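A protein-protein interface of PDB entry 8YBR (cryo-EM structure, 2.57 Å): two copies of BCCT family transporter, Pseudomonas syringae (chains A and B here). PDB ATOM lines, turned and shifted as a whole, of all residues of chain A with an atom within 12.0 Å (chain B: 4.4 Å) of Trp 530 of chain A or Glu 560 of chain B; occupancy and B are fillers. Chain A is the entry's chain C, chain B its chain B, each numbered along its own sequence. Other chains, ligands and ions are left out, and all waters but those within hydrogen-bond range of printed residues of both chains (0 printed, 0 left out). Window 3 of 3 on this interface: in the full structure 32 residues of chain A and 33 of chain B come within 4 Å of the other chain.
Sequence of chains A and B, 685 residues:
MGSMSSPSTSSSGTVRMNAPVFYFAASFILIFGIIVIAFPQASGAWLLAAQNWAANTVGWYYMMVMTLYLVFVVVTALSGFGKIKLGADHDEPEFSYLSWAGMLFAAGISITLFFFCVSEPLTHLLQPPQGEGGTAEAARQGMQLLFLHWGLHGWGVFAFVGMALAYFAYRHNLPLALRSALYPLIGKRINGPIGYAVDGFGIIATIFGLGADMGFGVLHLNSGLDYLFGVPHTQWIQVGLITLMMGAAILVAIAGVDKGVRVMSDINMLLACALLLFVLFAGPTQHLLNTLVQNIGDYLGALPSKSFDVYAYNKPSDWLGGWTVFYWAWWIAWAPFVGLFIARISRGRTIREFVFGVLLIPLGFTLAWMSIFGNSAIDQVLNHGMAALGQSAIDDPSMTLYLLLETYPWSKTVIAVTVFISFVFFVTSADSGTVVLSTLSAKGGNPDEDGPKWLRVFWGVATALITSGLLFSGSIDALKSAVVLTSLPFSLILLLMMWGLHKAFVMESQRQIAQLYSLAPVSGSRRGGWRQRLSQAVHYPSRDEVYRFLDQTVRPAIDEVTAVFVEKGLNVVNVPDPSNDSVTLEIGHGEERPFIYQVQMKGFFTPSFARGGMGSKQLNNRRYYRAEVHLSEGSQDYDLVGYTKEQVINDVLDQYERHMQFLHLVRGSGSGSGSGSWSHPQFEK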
ATOM      1  N   GLY A 524     -34.032   0.074  32.000  1.00  0.00           N
ATOM      2  CA  GLY A 524     -32.716  -0.106  31.418  1.00  0.00           C
ATOM      3  C   GLY A 524     -32.181   1.166  30.793  1.00  0.00           C
ATOM      4  O   GLY A 524     -30.968   1.320  30.610  1.00  0.00           O
ATOM      5  N   SER A 525     -33.085   2.090  30.465  1.00  0.00           N
ATOM      6  CA  SER A 525     -32.676   3.401  29.978  1.00  0.00           C
ATOM      7  C   SER A 525     -31.934   4.210  31.029  1.00  0.00           C
ATOM      8  O   SER A 525     -31.300   5.212  30.687  1.00  0.00           O
ATOM      9  CB  SER A 525     -33.890   4.189  29.502  1.00  0.00           C
ATOM     10  OG  SER A 525     -34.763   4.445  30.588  1.00  0.00           O
ATOM     11  N   ARG A 526     -32.019   3.821  32.300  1.00  0.00           N
ATOM     12  CA  ARG A 526     -31.254   4.516  33.326  1.00  0.00           C
ATOM     13  C   ARG A 526     -29.761   4.245  33.202  1.00  0.00           C
ATOM     14  O   ARG A 526     -28.960   4.985  33.787  1.00  0.00           O
ATOM     15  CB  ARG A 526     -31.750   4.122  34.718  1.00  0.00           C
ATOM     16  N   ARG A 527     -29.372   3.207  32.456  1.00  0.00           N
ATOM     17  CA  ARG A 527     -27.955   2.930  32.245  1.00  0.00           C
ATOM     18  C   ARG A 527     -27.263   4.098  31.555  1.00  0.00           C
ATOM     19  O   ARG A 527     -26.070   4.340  31.773  1.00  0.00           O
ATOM     20  CB  ARG A 527     -27.788   1.648  31.429  1.00  0.00           C
ATOM     21  N   GLY A 528     -27.991   4.829  30.718  1.00  0.00           N
ATOM     22  CA  GLY A 528     -27.477   6.037  30.110  1.00  0.00           C
ATOM     23  C   GLY A 528     -26.629   5.776  28.878  1.00  0.00           C
ATOM     24  O   GLY A 528     -26.152   4.670  28.619  1.00  0.00           O
ATOM     25  N   GLY A 529     -26.447   6.837  28.101  1.00  0.00           N
ATOM     26  CA  GLY A 529     -25.638   6.781  26.902  1.00  0.00           C
ATOM     27  C   GLY A 529     -26.494   6.647  25.663  1.00  0.00           C
ATOM     28  O   GLY A 529     -26.946   5.547  25.336  1.00  0.00           O
ATOM     29  N   TRP A 530     -26.724   7.755  24.959  1.00  0.00           N
ATOM     30  CA  TRP A 530     -27.538   7.689  23.754  1.00  0.00           C
ATOM     31  C   TRP A 530     -26.759   7.159  22.560  1.00  0.00           C
ATOM     32  O   TRP A 530     -27.370   6.777  21.558  1.00  0.00           O
ATOM     33  CB  TRP A 530     -28.129   9.065  23.435  1.00  0.00           C
ATOM     34  CG  TRP A 530     -27.189  10.003  22.742  1.00  0.00           C
ATOM     35  CD1 TRP A 530     -26.328  10.879  23.329  1.00  0.00           C
ATOM     36  CD2 TRP A 530     -27.033  10.170  21.330  1.00  0.00           C
ATOM     37  NE1 TRP A 530     -25.637  11.577  22.371  1.00  0.00           N
ATOM     38  CE2 TRP A 530     -26.052  11.159  21.135  1.00  0.00           C
ATOM     39  CE3 TRP A 530     -27.622   9.575  20.213  1.00  0.00           C
ATOM     40  CZ2 TRP A 530     -25.650  11.567  19.868  1.00  0.00           C
ATOM     41  CZ3 TRP A 530     -27.222   9.982  18.957  1.00  0.00           C
ATOM     42  CH2 TRP A 530     -26.245  10.968  18.795  1.00  0.00           C
ATOM     43  N   ARG A 531     -25.431   7.119  22.650  1.00  0.00           N
ATOM     44  CA  ARG A 531     -24.614   6.585  21.569  1.00  0.00           C
ATOM     45  C   ARG A 531     -24.351   5.095  21.720  1.00  0.00           C
ATOM     46  O   ARG A 531     -24.268   4.383  20.713  1.00  0.00           O
ATOM     47  CB  ARG A 531     -23.287   7.342  21.492  1.00  0.00           C
ATOM     48  CG  ARG A 531     -22.461   7.016  20.265  1.00  0.00           C
ATOM     49  CD  ARG A 531     -21.356   8.033  20.051  1.00  0.00           C
ATOM     50  NE  ARG A 531     -21.829   9.219  19.345  1.00  0.00           N
ATOM     51  CZ  ARG A 531     -22.078  10.387  19.927  1.00  0.00           C
ATOM     52  NH1 ARG A 531     -21.899  10.533  21.232  1.00  0.00           N
ATOM     53  NH2 ARG A 531     -22.504  11.412  19.203  1.00  0.00           N
ATOM     54  N   GLN A 532     -24.225   4.606  22.953  1.00  0.00           N
ATOM     55  CA  GLN A 532     -24.045   3.182  23.193  1.00  0.00           C
ATOM     56  C   GLN A 532     -25.361   2.421  23.180  1.00  0.00           C
ATOM     57  O   GLN A 532     -25.378   1.231  22.846  1.00  0.00           O
ATOM     58  CB  GLN A 532     -23.332   2.956  24.531  1.00  0.00           C
ATOM     59  CG  GLN A 532     -21.902   3.476  24.569  1.00  0.00           C
ATOM     60  CD  GLN A 532     -21.826   4.965  24.842  1.00  0.00           C
ATOM     61  OE1 GLN A 532     -22.845   5.652  24.874  1.00  0.00           O
ATOM     62  NE2 GLN A 532     -20.615   5.471  25.037  1.00  0.00           N
ATOM     63  N   ARG A 533     -26.464   3.080  23.538  1.00  0.00           N
ATOM     64  CA  ARG A 533     -27.773   2.452  23.426  1.00  0.00           C
ATOM     65  C   ARG A 533     -28.243   2.378  21.983  1.00  0.00           C
ATOM     66  O   ARG A 533     -29.138   1.586  21.673  1.00  0.00           O
ATOM     67  CB  ARG A 533     -28.791   3.214  24.271  1.00  0.00           C
ATOM     68  CG  ARG A 533     -30.031   2.421  24.628  1.00  0.00           C
ATOM     69  CD  ARG A 533     -30.735   3.033  25.828  1.00  0.00           C
ATOM     70  NE  ARG A 533     -31.043   4.445  25.616  1.00  0.00           N
ATOM     71  CZ  ARG A 533     -32.249   4.910  25.311  1.00  0.00           C
ATOM     72  NH1 ARG A 533     -32.433   6.210  25.137  1.00  0.00           N
ATOM     73  NH2 ARG A 533     -33.273   4.077  25.181  1.00  0.00           N
ATOM     74  N   LEU A 534     -27.658   3.182  21.095  1.00  0.00           N
ATOM     75  CA  LEU A 534     -28.057   3.173  19.694  1.00  0.00           C
ATOM     76  C   LEU A 534     -27.338   2.080  18.916  1.00  0.00           C
ATOM     77  O   LEU A 534     -27.945   1.415  18.070  1.00  0.00           O
ATOM     78  CB  LEU A 534     -27.788   4.544  19.070  1.00  0.00           C
ATOM     79  CG  LEU A 534     -28.113   4.724  17.588  1.00  0.00           C
ATOM     80  CD1 LEU A 534     -29.507   4.215  17.275  1.00  0.00           C
ATOM     81  CD2 LEU A 534     -27.981   6.182  17.198  1.00  0.00           C
ATOM     82  N   SER A 535     -26.046   1.885  19.188  1.00  0.00           N
ATOM     83  CA  SER A 535     -25.285   0.839  18.513  1.00  0.00           C
ATOM     84  C   SER A 535     -25.802  -0.546  18.885  1.00  0.00           C
ATOM     85  O   SER A 535     -25.815  -1.462  18.055  1.00  0.00           O
ATOM     86  CB  SER A 535     -23.803   0.979  18.855  1.00  0.00           C
ATOM     87  OG  SER A 535     -23.585   0.787  20.240  1.00  0.00           O
ATOM     88  N   GLN A 536     -26.216  -0.716  20.138  1.00  0.00           N
ATOM     89  CA  GLN A 536     -26.765  -1.981  20.608  1.00  0.00           C
ATOM     90  C   GLN A 536     -28.145  -2.279  20.028  1.00  0.00           C
ATOM     91  O   GLN A 536     -28.550  -3.447  19.991  1.00  0.00           O
ATOM     92  CB  GLN A 536     -26.823  -1.950  22.138  1.00  0.00           C
ATOM     93  CG  GLN A 536     -28.096  -2.522  22.741  1.00  0.00           C
ATOM     94  CD  GLN A 536     -28.007  -2.737  24.236  1.00  0.00           C
ATOM     95  OE1 GLN A 536     -26.931  -2.680  24.824  1.00  0.00           O
ATOM     96  NE2 GLN A 536     -29.146  -3.012  24.855  1.00  0.00           N
ATOM     97  N   ALA A 537     -28.855  -1.269  19.538  1.00  0.00           N
ATOM     98  CA  ALA A 537     -30.237  -1.429  19.101  1.00  0.00           C
ATOM     99  C   ALA A 537     -30.366  -1.956  17.679  1.00  0.00           C
ATOM    100  O   ALA A 537     -31.485  -2.012  17.163  1.00  0.00           O
ATOM    101  CB  ALA A 537     -30.977  -0.096  19.223  1.00  0.00           C
ATOM    102  N   VAL A 538     -29.263  -2.331  17.036  1.00  0.00           N
ATOM    103  CA  VAL A 538     -29.301  -2.812  15.658  1.00  0.00           C
ATOM    104  C   VAL A 538     -28.488  -4.093  15.523  1.00  0.00           C
ATOM    105  O   VAL A 538     -28.228  -4.561  14.409  1.00  0.00           O
ATOM    106  CB  VAL A 538     -28.789  -1.738  14.682  1.00  0.00           C
ATOM    107  CG1 VAL A 538     -29.762  -0.574  14.614  1.00  0.00           C
ATOM    108  CG2 VAL A 538     -27.413  -1.261  15.109  1.00  0.00           C
ATOM    109  N   PRO B 556     -31.447  21.610  16.102  1.00  0.00           N
ATOM    110  CA  PRO B 556     -30.061  21.122  16.207  1.00  0.00           C
ATOM    111  C   PRO B 556     -29.937  19.707  16.747  1.00  0.00           C
ATOM    112  O   PRO B 556     -28.810  19.216  16.872  1.00  0.00           O
ATOM    113  CB  PRO B 556     -29.401  22.133  17.155  1.00  0.00           C
ATOM    114  CG  PRO B 556     -30.281  23.331  17.117  1.00  0.00           C
ATOM    115  CD  PRO B 556     -31.659  22.785  16.964  1.00  0.00           C
ATOM    116  N   ALA B 557     -31.043  19.040  17.076  1.00  0.00           N
ATOM    117  CA  ALA B 557     -31.017  17.668  17.566  1.00  0.00           C
ATOM    118  C   ALA B 557     -31.508  16.671  16.526  1.00  0.00           C
ATOM    119  O   ALA B 557     -30.881  15.631  16.317  1.00  0.00           O
ATOM    120  CB  ALA B 557     -31.857  17.544  18.840  1.00  0.00           C
ATOM    121  N   ILE B 558     -32.632  16.972  15.870  1.00  0.00           N
ATOM    122  CA  ILE B 558     -33.147  16.086  14.830  1.00  0.00           C
ATOM    123  C   ILE B 558     -32.124  15.918  13.713  1.00  0.00           C
ATOM    124  O   ILE B 558     -31.885  14.804  13.236  1.00  0.00           O
ATOM    125  CB  ILE B 558     -34.491  16.613  14.298  1.00  0.00           C
ATOM    126  CG1 ILE B 558     -35.523  16.659  15.424  1.00  0.00           C
ATOM    127  CG2 ILE B 558     -34.981  15.763  13.143  1.00  0.00           C
ATOM    128  CD1 ILE B 558     -35.891  15.302  15.966  1.00  0.00           C
ATOM    129  N   ASP B 559     -31.498  17.015  13.287  1.00  0.00           N
ATOM    130  CA  ASP B 559     -30.448  16.923  12.281  1.00  0.00           C
ATOM    131  C   ASP B 559     -29.150  16.348  12.833  1.00  0.00           C
ATOM    132  O   ASP B 559     -28.226  16.086  12.056  1.00  0.00           O
ATOM    133  CB  ASP B 559     -30.183  18.299  11.663  1.00  0.00           C
ATOM    134  CG  ASP B 559     -29.305  19.175  12.537  1.00  0.00           C
ATOM    135  OD1 ASP B 559     -29.403  19.079  13.777  1.00  0.00           O
ATOM    136  OD2 ASP B 559     -28.516  19.967  11.980  1.00  0.00           O
ATOM    137  N   GLU B 560     -29.055  16.146  14.146  1.00  0.00           N
ATOM    138  CA  GLU B 560     -27.845  15.634  14.776  1.00  0.00           C
ATOM    139  C   GLU B 560     -27.943  14.160  15.137  1.00  0.00           C
ATOM    140  O   GLU B 560     -26.953  13.432  15.020  1.00  0.00           O
ATOM    141  CB  GLU B 560     -27.523  16.451  16.029  1.00  0.00           C
ATOM    142  CG  GLU B 560     -26.149  16.195  16.625  1.00  0.00           C
ATOM    143  CD  GLU B 560     -26.159  15.101  17.673  1.00  0.00           C
ATOM    144  OE1 GLU B 560     -27.211  14.903  18.314  1.00  0.00           O
ATOM    145  OE2 GLU B 560     -25.115  14.443  17.859  1.00  0.00           O
ATOM    146  N   VAL B 561     -29.118  13.702  15.574  1.00  0.00           N
ATOM    147  CA  VAL B 561     -29.277  12.287  15.884  1.00  0.00           C
ATOM    148  C   VAL B 561     -29.322  11.463  14.606  1.00  0.00           C
ATOM    149  O   VAL B 561     -28.835  10.328  14.575  1.00  0.00           O
ATOM    150  CB  VAL B 561     -30.529  12.068  16.757  1.00  0.00           C
ATOM    151  CG1 VAL B 561     -31.800  12.380  15.981  1.00  0.00           C
ATOM    152  CG2 VAL B 561     -30.567  10.649  17.290  1.00  0.00           C
ATOM    153  N   THR B 562     -29.876  12.019  13.524  1.00  0.00           N
ATOM    154  CA  THR B 562     -29.951  11.293  12.263  1.00  0.00           C
ATOM    155  C   THR B 562     -28.592  11.132  11.604  1.00  0.00           C
ATOM    156  O   THR B 562     -28.439  10.253  10.751  1.00  0.00           O
ATOM    157  CB  THR B 562     -30.906  11.997  11.300  1.00  0.00           C
ATOM    158  OG1 THR B 562     -31.063  11.185  10.131  1.00  0.00           O
ATOM    159  CG2 THR B 562     -30.345  13.347  10.888  1.00  0.00           C
ATOM    160  N   ALA B 563     -27.614  11.965  11.962  1.00  0.00           N
ATOM    161  CA  ALA B 563     -26.273  11.796  11.416  1.00  0.00           C
ATOM    162  C   ALA B 563     -25.726  10.417  11.746  1.00  0.00           C
ATOM    163  O   ALA B 563     -25.174   9.734  10.878  1.00  0.00           O
ATOM    164  CB  ALA B 563     -25.349  12.885  11.951  1.00  0.00           C
ATOM    165  N   VAL B 564     -25.883   9.985  12.997  1.00  0.00           N
ATOM    166  CA  VAL B 564     -25.457   8.653  13.387  1.00  0.00           C
ATOM    167  C   VAL B 564     -26.280   7.583  12.688  1.00  0.00           C
ATOM    168  O   VAL B 564     -25.811   6.453  12.528  1.00  0.00           O
ATOM    169  CB  VAL B 564     -25.544   8.510  14.918  1.00  0.00           C
ATOM    170  CG1 VAL B 564     -24.788   7.273  15.390  1.00  0.00           C
ATOM    171  CG2 VAL B 564     -25.015   9.763  15.600  1.00  0.00           C
ATOM    172  N   ILE B 649     -32.876  14.186  22.552  1.00  0.00           N
ATOM    173  CA  ILE B 649     -32.279  13.070  21.826  1.00  0.00           C
ATOM    174  C   ILE B 649     -32.565  11.756  22.538  1.00  0.00           C
ATOM    175  O   ILE B 649     -32.751  10.720  21.892  1.00  0.00           O
ATOM    176  CB  ILE B 649     -30.769  13.306  21.638  1.00  0.00           C
ATOM    177  CG1 ILE B 649     -30.530  14.445  20.646  1.00  0.00           C
ATOM    178  CG2 ILE B 649     -30.080  12.047  21.163  1.00  0.00           C
ATOM    179  CD1 ILE B 649     -29.271  15.231  20.909  1.00  0.00           C
ATOM    180  N   ASN B 650     -32.635  11.772  23.867  1.00  0.00           N
ATOM    181  CA  ASN B 650     -32.963  10.568  24.618  1.00  0.00           C
ATOM    182  C   ASN B 650     -34.446  10.232  24.576  1.00  0.00           C
ATOM    183  O   ASN B 650     -34.838   9.177  25.082  1.00  0.00           O
ATOM    184  CB  ASN B 650     -32.508  10.710  26.068  1.00  0.00           C
ATOM    185  CG  ASN B 650     -31.054  10.341  26.257  1.00  0.00           C
ATOM    186  OD1 ASN B 650     -30.182  11.207  26.290  1.00  0.00           O
ATOM    187  ND2 ASN B 650     -30.783   9.048  26.378  1.00  0.00           N
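Trp 530 of chain A touches Glu 560 of chain B.
Trp 530 of chain A touches Val 561 of chain B (CZ3 to CG2, 3.8 Å).
Trp 530 of chain A touches Val 564 of chain B.
Ile 649 of chain B touches Trp 530 of chain A.
ND2 of Asn 650 of chain B touches CB of Trp 530 of chain A, 3.96 Å away.
NH1 of Arg 533 of chain A touches ND2 of Asn 650 of chain B, 3.5 Å away.
CD2 of Leu 534 of chain A touches CG1 of Val 564 of chain B, 3.8 Å away.
Trp 530 of chain A touches just these residues of chain B: Glu 560 (3.5 Å), Val 561 (3.8 Å), Val 564 (3.6 Å), Ile 649 (3.6 Å) and Asn 650 (3.96 Å).
Of chain A, only Trp 530 comes within 4 Å of Glu 560 of chain B.
No residue of chain A comes within 4 Å of Pro 556 of chain B.
No residue of chain A comes within 4 Å of Ala 557 of chain B.
No residue of chain A comes within 4 Å of Ile 558 of chain B.
Val 561 of chain B touches just one residue of chain A: Trp 530 (3.8 Å).
No residue of chain A comes within 4 Å of Thr 562 of chain B.
No residue of chain A comes within 4 Å of Ala 563 of chain B.
Val 564 of chain B touches two residues of chain A.
Ile 649 of chain B touches just one residue of chain A: Trp 530 (3.6 Å).
Of chain A, only Trp 530 and Arg 533 come within 4 Å of Asn 650 of chain B.
Of the printed residues of chain B, Arg 533 of chain A touches Asn 650.
Of the printed residues of chain B, Leu 534 of chain A touches Val 564 (3.8 Å).
Ser 525 of chain A touches none of the printed residues of chain B.
Among the printed residues, 7 pairs touch across the chains.
Among the printed residues, no Asp or Glu carboxylate lies within 4 Å of a Lys or Arg side-chain nitrogen of the other chain.
No position is printed for both chains.
Of the 7 pairs that touch across the chains among the printed residues, none has its exchanged pair printed and touching as well.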
